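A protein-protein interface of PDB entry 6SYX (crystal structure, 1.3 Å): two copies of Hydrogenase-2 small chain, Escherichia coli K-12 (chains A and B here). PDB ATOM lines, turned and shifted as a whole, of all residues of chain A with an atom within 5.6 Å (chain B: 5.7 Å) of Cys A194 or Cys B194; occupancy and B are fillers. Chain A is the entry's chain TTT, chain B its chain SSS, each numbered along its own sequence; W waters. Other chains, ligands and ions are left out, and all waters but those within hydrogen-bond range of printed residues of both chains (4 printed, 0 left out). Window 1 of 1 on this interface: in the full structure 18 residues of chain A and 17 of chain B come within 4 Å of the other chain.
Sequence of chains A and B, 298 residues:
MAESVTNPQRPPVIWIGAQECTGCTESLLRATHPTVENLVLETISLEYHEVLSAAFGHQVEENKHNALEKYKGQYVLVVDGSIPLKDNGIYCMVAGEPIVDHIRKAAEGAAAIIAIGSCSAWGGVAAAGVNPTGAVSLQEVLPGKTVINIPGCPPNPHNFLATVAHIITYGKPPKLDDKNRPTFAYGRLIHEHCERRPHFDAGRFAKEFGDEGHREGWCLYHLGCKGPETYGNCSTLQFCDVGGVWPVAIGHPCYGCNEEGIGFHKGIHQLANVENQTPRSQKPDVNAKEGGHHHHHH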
ATOM      1  N   ILE A 190      19.478   0.820 -23.761  1.00  0.00           N
ATOM      2  CA  ILE A 190      19.245  -0.077 -24.924  1.00  0.00           C
ATOM      3  C   ILE A 190      17.990  -0.906 -24.658  1.00  0.00           C
ATOM      4  O   ILE A 190      17.164  -1.037 -25.577  1.00  0.00           O
ATOM      5  CB  ILE A 190      20.519  -0.904 -25.200  1.00  0.00           C
ATOM      6  CG1 ILE A 190      21.634   0.002 -25.724  1.00  0.00           C
ATOM      7  CG2 ILE A 190      20.206  -2.084 -26.124  1.00  0.00           C
ATOM      8  CD1 ILE A 190      23.030  -0.682 -25.775  1.00  0.00           C
ATOM      9  N   HIS A 191      17.817  -1.464 -23.431  1.00  0.00           N
ATOM     10  CA  HIS A 191      16.638  -2.290 -23.068  1.00  0.00           C
ATOM     11  C   HIS A 191      15.305  -1.531 -23.114  1.00  0.00           C
ATOM     12  O   HIS A 191      14.248  -2.206 -23.187  1.00  0.00           O
ATOM     13  CB  HIS A 191      16.905  -2.900 -21.688  1.00  0.00           C
ATOM     14  CG  HIS A 191      15.856  -3.796 -21.136  1.00  0.00           C
ATOM     15  ND1 HIS A 191      15.713  -5.108 -21.491  1.00  0.00           N
ATOM     16  CD2 HIS A 191      14.949  -3.587 -20.116  1.00  0.00           C
ATOM     17  CE1 HIS A 191      14.733  -5.648 -20.770  1.00  0.00           C
ATOM     18  NE2 HIS A 191      14.263  -4.720 -19.914  1.00  0.00           N
ATOM     19  N   GLU A 192      15.348  -0.200 -23.069  1.00  0.00           N
ATOM     20  CA  GLU A 192      14.128   0.662 -23.149  1.00  0.00           C
ATOM     21  C   GLU A 192      13.849   1.051 -24.610  1.00  0.00           C
ATOM     22  O   GLU A 192      12.878   1.831 -24.869  1.00  0.00           O
ATOM     23  CB  GLU A 192      14.208   1.867 -22.206  1.00  0.00           C
ATOM     24  CG  GLU A 192      14.157   1.442 -20.719  1.00  0.00           C
ATOM     25  CD  GLU A 192      12.934   0.632 -20.343  1.00  0.00           C
ATOM     26  OE1 GLU A 192      11.784   1.125 -20.658  1.00  0.00           O
ATOM     27  OE2 GLU A 192      13.040  -0.475 -19.769  1.00  0.00           O
ATOM     28  N   HIS A 193      14.531   0.418 -25.580  1.00  0.00           N
ATOM     29  CA  HIS A 193      14.216   0.589 -27.040  1.00  0.00           C
ATOM     30  C   HIS A 193      14.736  -0.629 -27.812  1.00  0.00           C
ATOM     31  O   HIS A 193      15.252  -0.434 -28.954  1.00  0.00           O
ATOM     32  CB  HIS A 193      14.733   1.946 -27.562  1.00  0.00           C
ATOM     33  CG  HIS A 193      13.895   2.577 -28.648  1.00  0.00           C
ATOM     34  ND1 HIS A 193      13.132   3.727 -28.458  1.00  0.00           N
ATOM     35  CD2 HIS A 193      13.663   2.165 -29.924  1.00  0.00           C
ATOM     36  CE1 HIS A 193      12.470   3.979 -29.601  1.00  0.00           C
ATOM     37  NE2 HIS A 193      12.786   3.042 -30.524  1.00  0.00           N
ATOM     38  N   CYS A 194      14.607  -1.841 -27.291  1.00  0.00           N
ATOM     39  CA  CYS A 194      15.100  -3.095 -27.902  1.00  0.00           C
ATOM     40  C   CYS A 194      13.947  -3.896 -28.502  1.00  0.00           C
ATOM     41  O   CYS A 194      12.929  -4.172 -27.793  1.00  0.00           O
ATOM     42  CB  CYS A 194      15.846  -3.951 -26.856  1.00  0.00           C
ATOM     43  SG  CYS A 194      16.471  -5.506 -27.578  1.00  0.00           S
ATOM     44  N   GLU A 195      14.109  -4.328 -29.751  1.00  0.00           N
ATOM     45  CA  GLU A 195      13.108  -5.129 -30.473  1.00  0.00           C
ATOM     46  C   GLU A 195      12.855  -6.517 -29.897  1.00  0.00           C
ATOM     47  O   GLU A 195      11.841  -7.141 -30.261  1.00  0.00           O
ATOM     48  CB  GLU A 195      13.423  -5.211 -31.965  1.00  0.00           C
ATOM     49  CG  GLU A 195      14.648  -6.018 -32.335  1.00  0.00           C
ATOM     50  CD  GLU A 195      16.014  -5.358 -32.299  1.00  0.00           C
ATOM     51  OE1 GLU A 195      16.155  -4.236 -31.696  1.00  0.00           O
ATOM     52  OE2 GLU A 195      16.941  -5.993 -32.913  1.00  0.00           O
ATOM     53  N   ARG A 196      13.723  -7.023 -28.987  1.00  0.00           N
ATOM     54  CA  ARG A 196      13.463  -8.325 -28.331  1.00  0.00           C
ATOM     55  C   ARG A 196      12.730  -8.163 -26.984  1.00  0.00           C
ATOM     56  O   ARG A 196      12.431  -9.180 -26.332  1.00  0.00           O
ATOM     57  CB  ARG A 196      14.773  -9.108 -28.176  1.00  0.00           C
ATOM     58  CG  ARG A 196      15.480  -9.319 -29.517  1.00  0.00           C
ATOM     59  CD  ARG A 196      16.533 -10.395 -29.520  1.00  0.00           C
ATOM     60  NE  ARG A 196      17.043 -10.528 -30.890  1.00  0.00           N
ATOM     61  CZ  ARG A 196      17.731 -11.583 -31.323  1.00  0.00           C
ATOM     62  NH1 ARG A 196      18.057 -12.586 -30.510  1.00  0.00           N
ATOM     63  NH2 ARG A 196      18.059 -11.646 -32.603  1.00  0.00           N
ATOM     64  N   ARG A 197      12.364  -6.965 -26.586  1.00  0.00           N
ATOM     65  CA  ARG A 197      11.593  -6.733 -25.324  1.00  0.00           C
ATOM     66  C   ARG A 197      10.331  -7.604 -25.270  1.00  0.00           C
ATOM     67  O   ARG A 197       9.982  -8.091 -24.178  1.00  0.00           O
ATOM     68  CB  ARG A 197      11.307  -5.244 -25.137  1.00  0.00           C
ATOM     69  CG  ARG A 197      10.529  -4.913 -23.860  1.00  0.00           C
ATOM     70  CD  ARG A 197      11.303  -5.272 -22.571  1.00  0.00           C
ATOM     71  NE  ARG A 197      10.575  -4.801 -21.379  1.00  0.00           N
ATOM     72  CZ  ARG A 197      10.720  -3.614 -20.852  1.00  0.00           C
ATOM     73  NH1 ARG A 197      11.685  -2.786 -21.221  1.00  0.00           N
ATOM     74  NH2 ARG A 197       9.835  -3.223 -19.921  1.00  0.00           N
ATOM     75  N   PRO A 198       9.542  -7.800 -26.357  1.00  0.00           N
ATOM     76  CA  PRO A 198       8.364  -8.695 -26.245  1.00  0.00           C
ATOM     77  C   PRO A 198       8.726 -10.087 -25.696  1.00  0.00           C
ATOM     78  O   PRO A 198       7.945 -10.738 -24.959  1.00  0.00           O
ATOM     79  CB  PRO A 198       7.840  -8.778 -27.697  1.00  0.00           C
ATOM     80  CG  PRO A 198       8.282  -7.460 -28.357  1.00  0.00           C
ATOM     81  CD  PRO A 198       9.661  -7.200 -27.722  1.00  0.00           C
ATOM     82  N   SER A 235      20.479  -0.351 -30.759  1.00  0.00           N
ATOM     83  CA  SER A 235      19.289  -1.073 -31.289  1.00  0.00           C
ATOM     84  C   SER A 235      18.590  -0.263 -32.389  1.00  0.00           C
ATOM     85  O   SER A 235      17.821  -0.938 -33.161  1.00  0.00           O
ATOM     86  CB  SER A 235      18.332  -1.444 -30.177  1.00  0.00           C
ATOM     87  OG  SER A 235      17.844  -0.207 -29.601  1.00  0.00           O
ATOM     88  N   TRP A 246      23.553  -5.184 -35.381  1.00  0.00           N
ATOM     89  CA  TRP A 246      24.077  -4.851 -34.039  1.00  0.00           C
ATOM     90  C   TRP A 246      24.310  -6.140 -33.274  1.00  0.00           C
ATOM     91  O   TRP A 246      23.854  -7.197 -33.760  1.00  0.00           O
ATOM     92  CB  TRP A 246      23.203  -3.846 -33.275  1.00  0.00           C
ATOM     93  CG  TRP A 246      21.847  -4.277 -32.739  1.00  0.00           C
ATOM     94  CD1 TRP A 246      20.692  -4.573 -33.448  1.00  0.00           C
ATOM     95  CD2 TRP A 246      21.464  -4.361 -31.350  1.00  0.00           C
ATOM     96  NE1 TRP A 246      19.653  -4.862 -32.603  1.00  0.00           N
ATOM     97  CE2 TRP A 246      20.104  -4.722 -31.299  1.00  0.00           C
ATOM     98  CE3 TRP A 246      22.146  -4.128 -30.139  1.00  0.00           C
ATOM     99  CZ2 TRP A 246      19.407  -4.792 -30.076  1.00  0.00           C
ATOM    100  CZ3 TRP A 246      21.455  -4.223 -28.942  1.00  0.00           C
ATOM    101  CH2 TRP A 246      20.106  -4.551 -28.929  1.00  0.00           C
ATOM    102  N   VAL A 248      23.161  -7.834 -30.632  1.00  0.00           N
ATOM    103  CA  VAL A 248      21.972  -8.647 -30.256  1.00  0.00           C
ATOM    104  C   VAL A 248      21.305  -9.190 -31.526  1.00  0.00           C
ATOM    105  O   VAL A 248      20.918 -10.401 -31.565  1.00  0.00           O
ATOM    106  CB  VAL A 248      21.011  -7.826 -29.355  1.00  0.00           C
ATOM    107  CG1 VAL A 248      19.617  -8.453 -29.252  1.00  0.00           C
ATOM    108  CG2 VAL A 248      21.642  -7.637 -27.942  1.00  0.00           C
ATOM    109  N   ILE B 190       4.270  -8.215 -35.695  1.00  0.00           N
ATOM    110  CA  ILE B 190       5.181  -7.057 -35.617  1.00  0.00           C
ATOM    111  C   ILE B 190       5.334  -6.628 -34.154  1.00  0.00           C
ATOM    112  O   ILE B 190       6.463  -6.368 -33.708  1.00  0.00           O
ATOM    113  CB  ILE B 190       4.700  -5.933 -36.573  1.00  0.00           C
ATOM    114  CG1 ILE B 190       4.854  -6.364 -38.032  1.00  0.00           C
ATOM    115  CG2 ILE B 190       5.374  -4.604 -36.289  1.00  0.00           C
ATOM    116  CD1 ILE B 190       4.208  -5.445 -39.052  1.00  0.00           C
ATOM    117  N   HIS B 191       4.235  -6.573 -33.382  1.00  0.00           N
ATOM    118  CA  HIS B 191       4.266  -6.157 -31.937  1.00  0.00           C
ATOM    119  C   HIS B 191       5.044  -7.148 -31.053  1.00  0.00           C
ATOM    120  O   HIS B 191       5.459  -6.723 -29.950  1.00  0.00           O
ATOM    121  CB  HIS B 191       2.819  -6.013 -31.442  1.00  0.00           C
ATOM    122  CG  HIS B 191       2.609  -5.554 -30.039  1.00  0.00           C
ATOM    123  ND1 HIS B 191       2.719  -4.250 -29.623  1.00  0.00           N
ATOM    124  CD2 HIS B 191       2.164  -6.254 -28.947  1.00  0.00           C
ATOM    125  CE1 HIS B 191       2.383  -4.196 -28.331  1.00  0.00           C
ATOM    126  NE2 HIS B 191       2.044  -5.386 -27.900  1.00  0.00           N
ATOM    127  N   GLU B 192       5.211  -8.392 -31.487  1.00  0.00           N
ATOM    128  CA  GLU B 192       6.031  -9.363 -30.724  1.00  0.00           C
ATOM    129  C   GLU B 192       7.514  -9.305 -31.164  1.00  0.00           C
ATOM    130  O   GLU B 192       8.335 -10.146 -30.664  1.00  0.00           O
ATOM    131  CB  GLU B 192       5.423 -10.751 -30.819  1.00  0.00           C
ATOM    132  CG  GLU B 192       4.059 -10.860 -30.110  1.00  0.00           C
ATOM    133  CD  GLU B 192       4.083 -10.526 -28.620  1.00  0.00           C
ATOM    134  OE1 GLU B 192       3.312  -9.648 -28.156  1.00  0.00           O
ATOM    135  OE2 GLU B 192       4.956 -11.079 -27.913  1.00  0.00           O
ATOM    136  N   HIS B 193       7.929  -8.281 -31.930  1.00  0.00           N
ATOM    137  CA  HIS B 193       9.371  -8.036 -32.232  1.00  0.00           C
ATOM    138  C   HIS B 193       9.567  -6.545 -32.549  1.00  0.00           C
ATOM    139  O   HIS B 193      10.375  -6.229 -33.447  1.00  0.00           O
ATOM    140  CB  HIS B 193       9.908  -8.991 -33.321  1.00  0.00           C
ATOM    141  CG  HIS B 193      11.346  -9.394 -33.155  1.00  0.00           C
ATOM    142  ND1 HIS B 193      11.717 -10.676 -32.796  1.00  0.00           N
ATOM    143  CD2 HIS B 193      12.481  -8.657 -33.303  1.00  0.00           C
ATOM    144  CE1 HIS B 193      13.063 -10.695 -32.708  1.00  0.00           C
ATOM    145  NE2 HIS B 193      13.554  -9.460 -33.008  1.00  0.00           N
ATOM    146  N   CYS B 194       8.934  -5.616 -31.826  1.00  0.00           N
ATOM    147  CA  CYS B 194       8.996  -4.168 -32.093  1.00  0.00           C
ATOM    148  C   CYS B 194       9.853  -3.463 -31.036  1.00  0.00           C
ATOM    149  O   CYS B 194       9.605  -3.657 -29.802  1.00  0.00           O
ATOM    150  CB  CYS B 194       7.590  -3.559 -32.065  1.00  0.00           C
ATOM    151  SG  CYS B 194       7.571  -1.760 -32.348  1.00  0.00           S
ATOM    152  N   GLU B 195      10.758  -2.592 -31.458  1.00  0.00           N
ATOM    153  CA  GLU B 195      11.685  -1.874 -30.570  1.00  0.00           C
ATOM    154  C   GLU B 195      10.984  -0.827 -29.700  1.00  0.00           C
ATOM    155  O   GLU B 195      11.629  -0.318 -28.746  1.00  0.00           O
ATOM    156  CB  GLU B 195      12.828  -1.279 -31.382  1.00  0.00           C
ATOM    157  CG  GLU B 195      12.469  -0.133 -32.347  1.00  0.00           C
ATOM    158  CD  GLU B 195      11.959  -0.458 -33.757  1.00  0.00           C
ATOM    159  OE1 GLU B 195      11.568  -1.634 -34.017  1.00  0.00           O
ATOM    160  OE2 GLU B 195      11.946   0.544 -34.599  1.00  0.00           O
ATOM    161  N   ARG B 196       9.693  -0.505 -29.960  1.00  0.00           N
ATOM    162  CA  ARG B 196       8.942   0.443 -29.103  1.00  0.00           C
ATOM    163  C   ARG B 196       8.156  -0.319 -28.034  1.00  0.00           C
ATOM    164  O   ARG B 196       7.480   0.351 -27.192  1.00  0.00           O
ATOM    165  CB  ARG B 196       8.066   1.427 -29.896  1.00  0.00           C
ATOM    166  CG  ARG B 196       8.891   2.158 -30.952  1.00  0.00           C
ATOM    167  CD  ARG B 196       8.239   3.382 -31.542  1.00  0.00           C
ATOM    168  NE  ARG B 196       9.185   4.098 -32.400  1.00  0.00           N
ATOM    169  CZ  ARG B 196       9.019   5.316 -32.847  1.00  0.00           C
ATOM    170  NH1 ARG B 196       7.939   6.041 -32.530  1.00  0.00           N
ATOM    171  NH2 ARG B 196       9.975   5.844 -33.596  1.00  0.00           N
ATOM    172  N   ARG B 197       8.261  -1.638 -27.948  1.00  0.00           N
ATOM    173  CA  ARG B 197       7.502  -2.394 -26.907  1.00  0.00           C
ATOM    174  C   ARG B 197       7.853  -1.906 -25.496  1.00  0.00           C
ATOM    175  O   ARG B 197       6.929  -1.883 -24.658  1.00  0.00           O
ATOM    176  CB  ARG B 197       7.783  -3.891 -27.041  1.00  0.00           C
ATOM    177  CG  ARG B 197       7.051  -4.764 -26.014  1.00  0.00           C
ATOM    178  CD  ARG B 197       5.518  -4.679 -26.118  1.00  0.00           C
ATOM    179  NE  ARG B 197       4.911  -5.676 -25.198  1.00  0.00           N
ATOM    180  CZ  ARG B 197       4.648  -6.941 -25.526  1.00  0.00           C
ATOM    181  NH1 ARG B 197       4.685  -7.353 -26.776  1.00  0.00           N
ATOM    182  NH2 ARG B 197       4.301  -7.827 -24.593  1.00  0.00           N
ATOM    183  N   PRO B 198       9.099  -1.510 -25.127  1.00  0.00           N
ATOM    184  CA  PRO B 198       9.298  -0.978 -23.759  1.00  0.00           C
ATOM    185  C   PRO B 198       8.371   0.207 -23.443  1.00  0.00           C
ATOM    186  O   PRO B 198       7.987   0.385 -22.251  1.00  0.00           O
ATOM    187  CB  PRO B 198      10.770  -0.552 -23.766  1.00  0.00           C
ATOM    188  CG  PRO B 198      11.404  -1.432 -24.837  1.00  0.00           C
ATOM    189  CD  PRO B 198      10.344  -1.528 -25.927  1.00  0.00           C
ATOM    190  N   SER B 235       9.632  -4.612 -38.712  1.00  0.00           N
ATOM    191  CA  SER B 235      10.475  -4.025 -37.644  1.00  0.00           C
ATOM    192  C   SER B 235      11.924  -4.559 -37.682  1.00  0.00           C
ATOM    193  O   SER B 235      12.781  -3.881 -37.027  1.00  0.00           O
ATOM    194  CB  SER B 235       9.827  -4.269 -36.263  1.00  0.00           C
ATOM    195  OG  SER B 235       9.813  -5.703 -36.010  1.00  0.00           O
ATOM    196  N   TRP B 246      11.311   1.977 -41.473  1.00  0.00           N
ATOM    197  CA  TRP B 246       9.981   1.327 -41.588  1.00  0.00           C
ATOM    198  C   TRP B 246       8.957   2.344 -41.095  1.00  0.00           C
ATOM    199  O   TRP B 246       9.363   3.370 -40.478  1.00  0.00           O
ATOM    200  CB  TRP B 246       9.924  -0.041 -40.864  1.00  0.00           C
ATOM    201  CG  TRP B 246       9.975  -0.070 -39.358  1.00  0.00           C
ATOM    202  CD1 TRP B 246      11.026   0.206 -38.504  1.00  0.00           C
ATOM    203  CD2 TRP B 246       8.894  -0.550 -38.499  1.00  0.00           C
ATOM    204  NE1 TRP B 246      10.693  -0.098 -37.205  1.00  0.00           N
ATOM    205  CE2 TRP B 246       9.386  -0.537 -37.161  1.00  0.00           C
ATOM    206  CE3 TRP B 246       7.603  -1.043 -38.730  1.00  0.00           C
ATOM    207  CZ2 TRP B 246       8.612  -1.004 -36.081  1.00  0.00           C
ATOM    208  CZ3 TRP B 246       6.837  -1.464 -37.657  1.00  0.00           C
ATOM    209  CH2 TRP B 246       7.365  -1.486 -36.357  1.00  0.00           C
ATOM    210  N   VAL B 248       6.817   2.780 -38.555  1.00  0.00           N
ATOM    211  CA  VAL B 248       6.818   3.160 -37.104  1.00  0.00           C
ATOM    212  C   VAL B 248       8.102   3.925 -36.796  1.00  0.00           C
ATOM    213  O   VAL B 248       8.050   4.985 -36.114  1.00  0.00           O
ATOM    214  CB  VAL B 248       6.642   1.923 -36.225  1.00  0.00           C
ATOM    215  CG1 VAL B 248       7.055   2.211 -34.788  1.00  0.00           C
ATOM    216  CG2 VAL B 248       5.194   1.420 -36.301  1.00  0.00           C
HETATM  217  O   HOH W   1       9.560  -0.245 -19.979  1.00  0.00           O
HETATM  218  O   HOH W   2      16.465  -8.763 -33.272  1.00  0.00           O
HETATM  219  O   HOH W   3      11.814   3.061 -33.344  1.00  0.00           O
HETATM  220  O   HOH W   4       5.104 -10.600 -25.279  1.00  0.00           O
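O of His A191 touches CG of Pro B198 (3.4 Å). Glu B195 touches His A193 (O to CA, 3.2 Å). Pro B198 touches His A193. Glu A195 touches Cys B194. Glu B195 touches Glu A195 (CA to N, 3.5 Å). NE2 of His B193 touches CG of Arg A196, at 3.99 Å. Pro A198 touches Glu B192. CG of Pro A198 touches N of His B193, at 3.7 Å. Cys B194 touches Pro A198. Pro A198 touches Arg B197.
Of the 12 printed residues of chain A, 8 touch a printed residue of chain B. Hydrophobic or aromatic side chains of chain A that line the printed part of chain B: His A193 and Pro A198. Hydrophobic or aromatic side chains of chain B that line the printed part of chain A: His B193 and Pro B198. Among the printed residues, no Asp or Glu carboxylate lies within 4 Å of a Lys or Arg side-chain nitrogen of the other chain.
OE2 of Glu A192 is in salt-bridge range of NH1 of Arg A197, at 3.0 Å. N of Arg A196 sits close to SG of Cys A194, 3.4 Å away. O of His A191 lies within hydrogen-bond range of NH1 of Arg A197 (3.3 Å). The indole nitrogen (NE1) of Trp A246 lies within hydrogen-bond range of the side-chain carboxylate (OE2) of Glu A195 (3.0 Å). The backbone carbonyl oxygen of His B193 lies within hydrogen-bond range of the side-chain hydroxyl of Ser B235 (2.7 Å). The guanidinium group (NH2) of Arg A196 sits at hydrogen-bond distance from the backbone carbonyl oxygen (O) of Val A248, 3.3 Å away.
Water W4 lies within hydrogen-bond range of OE2 of Glu B192, O of Pro A198 and NH2 of Arg B197. Water W1 lies within hydrogen-bond range of OE1 of Glu A192 (2.7 Å), O of Pro B198 (2.8 Å) and NH2 of Arg A197 (3.0 Å). Water W3 lies within hydrogen-bond range of OE2 of Glu B195 (2.8 Å), NE of Arg B196 (3.0 Å) and NE2 of His A193 (3.0 Å). Water W2 lies within hydrogen-bond range of the side-chain carboxylate of Glu A195 (2.8 Å), a ring nitrogen (NE2) of His B193 (3.0 Å) and the guanidinium group of Arg A196 (3.0 Å).
His A191 touches Pro B198, and with the chains exchanged Pro A198 touches His B191. Glu A192 touches Pro B198, and with the chains exchanged Pro A198 touches Glu B192. His A193 touches Pro B198, and with the chains exchanged Pro A198 touches His B193. Cys A194 touches its own counterpart, Cys B194. Of the 16 pairs that touch across the chains among the printed residues, 14 have their exchanged pair printed and touching as well.
Cys A194 touches just these residues of chain B: Cys B194 (3.9 Å) and Glu B195 (3.6 Å). Of the printed residues of chain A, Cys B194 touches Cys A194 (3.9 Å), Glu A195 (3.6 Å) and Pro A198 (3.98 Å). Of the printed residues of chain A, Glu B192 touches Pro A198. Printed residues of chain B within 4 Å of His A193: Glu B195 (3.2 Å) and Pro B198 (3.7 Å).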
